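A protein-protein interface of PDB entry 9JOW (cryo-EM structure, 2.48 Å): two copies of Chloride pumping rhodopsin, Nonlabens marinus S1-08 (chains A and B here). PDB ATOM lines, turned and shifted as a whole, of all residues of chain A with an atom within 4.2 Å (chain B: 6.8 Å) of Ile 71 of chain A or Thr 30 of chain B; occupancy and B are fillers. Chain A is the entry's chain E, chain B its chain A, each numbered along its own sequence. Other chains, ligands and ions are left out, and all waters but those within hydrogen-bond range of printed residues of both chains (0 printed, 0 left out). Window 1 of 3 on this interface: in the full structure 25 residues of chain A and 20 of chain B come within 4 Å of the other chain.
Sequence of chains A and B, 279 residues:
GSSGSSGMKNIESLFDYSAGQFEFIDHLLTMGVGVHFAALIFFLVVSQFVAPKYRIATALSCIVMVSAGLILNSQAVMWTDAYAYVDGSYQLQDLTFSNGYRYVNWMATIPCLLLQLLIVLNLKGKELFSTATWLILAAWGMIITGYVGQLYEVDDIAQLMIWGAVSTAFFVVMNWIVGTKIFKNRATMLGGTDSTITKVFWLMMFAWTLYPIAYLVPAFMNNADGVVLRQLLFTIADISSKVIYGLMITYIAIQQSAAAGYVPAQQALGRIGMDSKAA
The side-chain hydroxyl (OG1) of Thr 30 of chain B lies within hydrogen-bond range of the backbone carbonyl oxygen (O) of Asp 26 of chain B, at 2.9 Å.
ND2 of Asn 105 of chain A is in hydrogen-bond range of OG of Ser 67 of chain A, at 3.0 Å.
ND1 of His 27 of chain B is in hydrogen-bond range of N of Tyr 101 of chain A.
The side-chain carboxylate of Asp 26 of chain B lies close to the side-chain hydroxyl of Tyr 101 of chain A (2.2 Å).
1 position is printed for both chains.
Of the 11 printed residues of chain A, 5 touch a printed residue of chain B.
Hydrophobic or aromatic side chains of chain A within 4 Å of the printed part of chain B: Leu 70, Ile 71 and Tyr 101.
Printed residues of chain B that touch a printed residue of chain A: Asp 26, His 27, Thr 30, Met 31 and Gly 34.
Among the printed residues, no Asp or Glu carboxylate lies within 4 Å of a Lys or Arg side-chain nitrogen of the other chain.
Leu 70 of chain A touches Gly 34 of chain B (CD1 to CA, 3.9 Å).
Thr 30 of chain B touches Ile 71 of chain A (CG2 to CD1, 3.7 Å).
Thr 30 of chain B touches Ser 74 of chain A.
Tyr 101 of chain A touches Thr 30 of chain B (CE2 to OG1, 3.7 Å).
Asn 105 of chain A touches Met 31 of chain B (OD1 to CG, 3.8 Å).
Ala 68 of chain A touches none of the printed residues of chain B.
Printed residues of chain B within 4 Å of Ile 71 of chain A: Thr 30 (3.7 Å).
Printed residues of chain B within 4 Å of Tyr 101 of chain A: Asp 26, His 27 and Thr 30.
Of the printed residues of chain B, Asn 105 of chain A touches Met 31 (3.8 Å).
Printed residues of chain A within 4 Å of Asp 26 of chain B: Tyr 101.
Thr 30 of chain B touches just these residues of chain A: Ile 71, Ser 74 and Tyr 101.
Printed residues of chain A within 4 Å of Met 31 of chain B: Asn 105.
Gly 32 of chain B touches none of the printed residues of chain A.
Of the printed residues of chain A, Gly 34 of chain B touches Leu 70 (3.9 Å).
The nearest printed residue of chain A that does not touch Thr 30 of chain B is Leu 70 of chain A (5.2 Å).
The nearest printed residue of chain A that does not touch Met 31 of chain B is Ile 71 of chain A (4.8 Å).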
ATOM      1  N   SER A  67      -5.715 -24.338  23.201  1.00  0.00           N
ATOM      2  CA  SER A  67      -4.968 -23.531  24.147  1.00  0.00           C
ATOM      3  C   SER A  67      -4.372 -24.412  25.253  1.00  0.00           C
ATOM      4  O   SER A  67      -3.171 -24.398  25.464  1.00  0.00           O
ATOM      5  CB  SER A  67      -5.872 -22.476  24.699  1.00  0.00           C
ATOM      6  OG  SER A  67      -5.344 -21.785  25.797  1.00  0.00           O
ATOM      7  N   ALA A  68      -5.175 -25.220  25.917  1.00  0.00           N
ATOM      8  CA  ALA A  68      -4.683 -26.155  26.919  1.00  0.00           C
ATOM      9  C   ALA A  68      -3.758 -27.220  26.330  1.00  0.00           C
ATOM     10  O   ALA A  68      -2.704 -27.504  26.856  1.00  0.00           O
ATOM     11  CB  ALA A  68      -5.857 -26.827  27.605  1.00  0.00           C
ATOM     12  N   GLY A  69      -4.071 -27.755  25.174  1.00  0.00           N
ATOM     13  CA  GLY A  69      -3.156 -28.685  24.529  1.00  0.00           C
ATOM     14  C   GLY A  69      -1.756 -28.129  24.332  1.00  0.00           C
ATOM     15  O   GLY A  69      -0.790 -28.824  24.593  1.00  0.00           O
ATOM     16  N   LEU A  70      -1.637 -26.896  23.839  1.00  0.00           N
ATOM     17  CA  LEU A  70      -0.322 -26.342  23.657  1.00  0.00           C
ATOM     18  C   LEU A  70       0.410 -26.002  24.982  1.00  0.00           C
ATOM     19  O   LEU A  70       1.628 -26.058  25.015  1.00  0.00           O
ATOM     20  CB  LEU A  70      -0.465 -25.110  22.810  1.00  0.00           C
ATOM     21  CG  LEU A  70      -0.841 -25.322  21.367  1.00  0.00           C
ATOM     22  CD1 LEU A  70      -1.017 -24.013  20.649  1.00  0.00           C
ATOM     23  CD2 LEU A  70       0.288 -26.013  20.792  1.00  0.00           C
ATOM     24  N   ILE A  71      -0.249 -25.599  26.048  1.00  0.00           N
ATOM     25  CA  ILE A  71       0.432 -25.406  27.331  1.00  0.00           C
ATOM     26  C   ILE A  71       0.930 -26.760  27.792  1.00  0.00           C
ATOM     27  O   ILE A  71       2.075 -26.887  28.213  1.00  0.00           O
ATOM     28  CB  ILE A  71      -0.473 -24.789  28.439  1.00  0.00           C
ATOM     29  CG1 ILE A  71      -0.837 -23.387  28.184  1.00  0.00           C
ATOM     30  CG2 ILE A  71       0.194 -24.811  29.806  1.00  0.00           C
ATOM     31  CD1 ILE A  71       0.375 -22.505  28.188  1.00  0.00           C
ATOM     32  N   LEU A  72       0.087 -27.785  27.780  1.00  0.00           N
ATOM     33  CA  LEU A  72       0.594 -29.080  28.205  1.00  0.00           C
ATOM     34  C   LEU A  72       1.810 -29.457  27.370  1.00  0.00           C
ATOM     35  O   LEU A  72       2.803 -29.946  27.863  1.00  0.00           O
ATOM     36  CB  LEU A  72      -0.460 -30.161  28.173  1.00  0.00           C
ATOM     37  CG  LEU A  72      -1.557 -29.976  29.233  1.00  0.00           C
ATOM     38  CD1 LEU A  72      -2.684 -30.979  29.040  1.00  0.00           C
ATOM     39  CD2 LEU A  72      -0.947 -30.137  30.576  1.00  0.00           C
ATOM     40  N   ASN A  73       1.781 -29.135  26.099  1.00  0.00           N
ATOM     41  CA  ASN A  73       2.872 -29.576  25.289  1.00  0.00           C
ATOM     42  C   ASN A  73       4.160 -28.881  25.699  1.00  0.00           C
ATOM     43  O   ASN A  73       5.213 -29.488  25.756  1.00  0.00           O
ATOM     44  CB  ASN A  73       2.510 -29.435  23.831  1.00  0.00           C
ATOM     45  CG  ASN A  73       3.693 -29.852  23.001  1.00  0.00           C
ATOM     46  OD1 ASN A  73       4.059 -31.023  22.975  1.00  0.00           O
ATOM     47  ND2 ASN A  73       4.389 -28.903  22.443  1.00  0.00           N
ATOM     48  N   SER A  74       4.073 -27.602  26.002  1.00  0.00           N
ATOM     49  CA  SER A  74       5.211 -26.869  26.543  1.00  0.00           C
ATOM     50  C   SER A  74       5.682 -27.481  27.860  1.00  0.00           C
ATOM     51  O   SER A  74       6.869 -27.642  28.025  1.00  0.00           O
ATOM     52  CB  SER A  74       4.899 -25.399  26.755  1.00  0.00           C
ATOM     53  OG  SER A  74       5.336 -24.616  25.664  1.00  0.00           O
ATOM     54  N   GLN A  75       4.789 -27.721  28.821  1.00  0.00           N
ATOM     55  CA  GLN A  75       5.253 -28.244  30.087  1.00  0.00           C
ATOM     56  C   GLN A  75       5.962 -29.580  29.871  1.00  0.00           C
ATOM     57  O   GLN A  75       6.968 -29.853  30.492  1.00  0.00           O
ATOM     58  CB  GLN A  75       4.116 -28.536  31.038  1.00  0.00           C
ATOM     59  CG  GLN A  75       3.453 -27.293  31.608  1.00  0.00           C
ATOM     60  CD  GLN A  75       4.265 -26.730  32.738  1.00  0.00           C
ATOM     61  OE1 GLN A  75       5.362 -26.210  32.531  1.00  0.00           O
ATOM     62  NE2 GLN A  75       3.767 -26.886  33.948  1.00  0.00           N
ATOM     63  N   TYR A 101       2.886 -21.479  33.916  1.00  0.00           N
ATOM     64  CA  TYR A 101       2.296 -21.595  32.590  1.00  0.00           C
ATOM     65  C   TYR A 101       0.792 -21.852  32.659  1.00  0.00           C
ATOM     66  O   TYR A 101       0.016 -21.220  31.952  1.00  0.00           O
ATOM     67  CB  TYR A 101       2.911 -22.725  31.779  1.00  0.00           C
ATOM     68  CG  TYR A 101       4.383 -22.457  31.557  1.00  0.00           C
ATOM     69  CD1 TYR A 101       5.300 -22.842  32.521  1.00  0.00           C
ATOM     70  CD2 TYR A 101       4.842 -21.730  30.468  1.00  0.00           C
ATOM     71  CE1 TYR A 101       6.650 -22.597  32.363  1.00  0.00           C
ATOM     72  CE2 TYR A 101       6.188 -21.445  30.318  1.00  0.00           C
ATOM     73  CZ  TYR A 101       7.098 -21.910  31.253  1.00  0.00           C
ATOM     74  OH  TYR A 101       8.440 -21.668  31.178  1.00  0.00           O
ATOM     75  N   ASN A 105      -2.446 -19.255  31.481  1.00  0.00           N
ATOM     76  CA  ASN A 105      -3.376 -19.762  30.495  1.00  0.00           C
ATOM     77  C   ASN A 105      -4.838 -19.749  30.946  1.00  0.00           C
ATOM     78  O   ASN A 105      -5.722 -19.505  30.132  1.00  0.00           O
ATOM     79  CB  ASN A 105      -3.040 -21.198  30.108  1.00  0.00           C
ATOM     80  CG  ASN A 105      -3.510 -21.415  28.705  1.00  0.00           C
ATOM     81  OD1 ASN A 105      -3.087 -20.658  27.807  1.00  0.00           O
ATOM     82  ND2 ASN A 105      -4.375 -22.406  28.516  1.00  0.00           N
ATOM     83  N   ILE B  25       8.149 -13.956  32.170  1.00  0.00           N
ATOM     84  CA  ILE B  25       8.201 -13.644  30.756  1.00  0.00           C
ATOM     85  C   ILE B  25       7.913 -14.889  29.928  1.00  0.00           C
ATOM     86  O   ILE B  25       7.143 -14.806  28.993  1.00  0.00           O
ATOM     87  CB  ILE B  25       9.528 -12.965  30.372  1.00  0.00           C
ATOM     88  CG1 ILE B  25       9.569 -11.530  30.910  1.00  0.00           C
ATOM     89  CG2 ILE B  25       9.701 -12.959  28.858  1.00  0.00           C
ATOM     90  CD1 ILE B  25      10.952 -10.947  30.892  1.00  0.00           C
ATOM     91  N   ASP B  26       8.480 -16.048  30.284  1.00  0.00           N
ATOM     92  CA  ASP B  26       8.170 -17.238  29.506  1.00  0.00           C
ATOM     93  C   ASP B  26       6.677 -17.609  29.607  1.00  0.00           C
ATOM     94  O   ASP B  26       6.102 -18.110  28.640  1.00  0.00           O
ATOM     95  CB  ASP B  26       9.057 -18.405  29.919  1.00  0.00           C
ATOM     96  CG  ASP B  26       9.093 -19.542  28.895  1.00  0.00           C
ATOM     97  OD1 ASP B  26       9.065 -19.244  27.666  1.00  0.00           O
ATOM     98  OD2 ASP B  26       9.161 -20.728  29.311  1.00  0.00           O
ATOM     99  N   HIS B  27       6.068 -17.434  30.798  1.00  0.00           N
ATOM    100  CA  HIS B  27       4.642 -17.645  30.940  1.00  0.00           C
ATOM    101  C   HIS B  27       3.839 -16.766  29.959  1.00  0.00           C
ATOM    102  O   HIS B  27       2.982 -17.264  29.276  1.00  0.00           O
ATOM    103  CB  HIS B  27       4.179 -17.385  32.371  1.00  0.00           C
ATOM    104  CG  HIS B  27       4.814 -18.238  33.387  1.00  0.00           C
ATOM    105  ND1 HIS B  27       5.387 -19.461  33.127  1.00  0.00           N
ATOM    106  CD2 HIS B  27       5.020 -17.987  34.704  1.00  0.00           C
ATOM    107  CE1 HIS B  27       5.943 -19.907  34.263  1.00  0.00           C
ATOM    108  NE2 HIS B  27       5.735 -19.034  35.230  1.00  0.00           N
ATOM    109  N   LEU B  28       4.133 -15.469  29.882  1.00  0.00           N
ATOM    110  CA  LEU B  28       3.439 -14.570  28.981  1.00  0.00           C
ATOM    111  C   LEU B  28       3.626 -14.970  27.523  1.00  0.00           C
ATOM    112  O   LEU B  28       2.660 -15.105  26.800  1.00  0.00           O
ATOM    113  CB  LEU B  28       3.942 -13.155  29.187  1.00  0.00           C
ATOM    114  CG  LEU B  28       3.559 -12.506  30.524  1.00  0.00           C
ATOM    115  CD1 LEU B  28       4.265 -11.168  30.637  1.00  0.00           C
ATOM    116  CD2 LEU B  28       2.081 -12.293  30.624  1.00  0.00           C
ATOM    117  N   LEU B  29       4.852 -15.166  27.074  1.00  0.00           N
ATOM    118  CA  LEU B  29       5.082 -15.565  25.693  1.00  0.00           C
ATOM    119  C   LEU B  29       4.344 -16.863  25.384  1.00  0.00           C
ATOM    120  O   LEU B  29       3.742 -17.001  24.332  1.00  0.00           O
ATOM    121  CB  LEU B  29       6.567 -15.706  25.338  1.00  0.00           C
ATOM    122  CG  LEU B  29       7.407 -14.444  25.549  1.00  0.00           C
ATOM    123  CD1 LEU B  29       8.876 -14.711  25.356  1.00  0.00           C
ATOM    124  CD2 LEU B  29       6.954 -13.381  24.630  1.00  0.00           C
ATOM    125  N   THR B  30       4.350 -17.818  26.298  1.00  0.00           N
ATOM    126  CA  THR B  30       3.773 -19.095  25.940  1.00  0.00           C
ATOM    127  C   THR B  30       2.249 -18.975  25.803  1.00  0.00           C
ATOM    128  O   THR B  30       1.631 -19.569  24.927  1.00  0.00           O
ATOM    129  CB  THR B  30       4.207 -20.144  26.949  1.00  0.00           C
ATOM    130  OG1 THR B  30       5.615 -20.312  26.863  1.00  0.00           O
ATOM    131  CG2 THR B  30       3.609 -21.493  26.652  1.00  0.00           C
ATOM    132  N   MET B  31       1.624 -18.181  26.628  1.00  0.00           N
ATOM    133  CA  MET B  31       0.182 -18.034  26.591  1.00  0.00           C
ATOM    134  C   MET B  31      -0.238 -17.375  25.282  1.00  0.00           C
ATOM    135  O   MET B  31      -1.129 -17.857  24.587  1.00  0.00           O
ATOM    136  CB  MET B  31      -0.256 -17.176  27.777  1.00  0.00           C
ATOM    137  CG  MET B  31      -1.722 -17.072  27.974  1.00  0.00           C
ATOM    138  SD  MET B  31      -2.237 -15.495  27.326  1.00  0.00           S
ATOM    139  CE  MET B  31      -1.513 -14.404  28.552  1.00  0.00           C
ATOM    140  N   GLY B  32       0.417 -16.293  24.936  1.00  0.00           N
ATOM    141  CA  GLY B  32       0.202 -15.642  23.658  1.00  0.00           C
ATOM    142  C   GLY B  32       0.186 -16.592  22.459  1.00  0.00           C
ATOM    143  O   GLY B  32      -0.720 -16.513  21.655  1.00  0.00           O
ATOM    144  N   VAL B  33       1.104 -17.540  22.369  1.00  0.00           N
ATOM    145  CA  VAL B  33       1.069 -18.460  21.252  1.00  0.00           C
ATOM    146  C   VAL B  33      -0.258 -19.204  21.156  1.00  0.00           C
ATOM    147  O   VAL B  33      -0.844 -19.336  20.080  1.00  0.00           O
ATOM    148  CB  VAL B  33       2.180 -19.503  21.276  1.00  0.00           C
ATOM    149  CG1 VAL B  33       1.990 -20.517  20.127  1.00  0.00           C
ATOM    150  CG2 VAL B  33       3.544 -18.821  21.215  1.00  0.00           C
ATOM    151  N   GLY B  34      -0.761 -19.688  22.267  1.00  0.00           N
ATOM    152  CA  GLY B  34      -1.930 -20.559  22.201  1.00  0.00           C
ATOM    153  C   GLY B  34      -3.242 -19.783  22.042  1.00  0.00           C
ATOM    154  O   GLY B  34      -4.167 -20.231  21.373  1.00  0.00           O
ATOM    155  N   VAL B  35      -3.334 -18.600  22.637  1.00  0.00           N
ATOM    156  CA  VAL B  35      -4.502 -17.798  22.388  1.00  0.00           C
ATOM    157  C   VAL B  35      -4.600 -17.507  20.884  1.00  0.00           C
ATOM    158  O   VAL B  35      -5.687 -17.621  20.324  1.00  0.00           O
ATOM    159  CB  VAL B  35      -4.492 -16.525  23.248  1.00  0.00           C
ATOM    160  CG1 VAL B  35      -5.611 -15.594  22.900  1.00  0.00           C
ATOM    161  CG2 VAL B  35      -4.665 -16.885  24.696  1.00  0.00           C
ATOM    162  N   LEU B  72       5.046 -15.310  17.810  1.00  0.00           N
ATOM    163  CA  LEU B  72       5.150 -15.538  19.238  1.00  0.00           C
ATOM    164  C   LEU B  72       5.843 -16.858  19.473  1.00  0.00           C
ATOM    165  O   LEU B  72       6.670 -16.998  20.364  1.00  0.00           O
ATOM    166  CB  LEU B  72       3.823 -15.452  19.977  1.00  0.00           C
ATOM    167  CG  LEU B  72       3.248 -14.033  20.011  1.00  0.00           C
ATOM    168  CD1 LEU B  72       1.821 -14.044  20.539  1.00  0.00           C
ATOM    169  CD2 LEU B  72       4.139 -13.198  20.855  1.00  0.00           C
ATOM    170  N   ALA B  76       9.162 -17.311  21.787  1.00  0.00           N
ATOM    171  CA  ALA B  76       9.085 -18.047  23.032  1.00  0.00           C
ATOM    172  C   ALA B  76      10.185 -19.089  23.062  1.00  0.00           C
ATOM    173  O   ALA B  76      10.688 -19.384  24.136  1.00  0.00           O
ATOM    174  CB  ALA B  76       7.741 -18.713  23.195  1.00  0.00           C
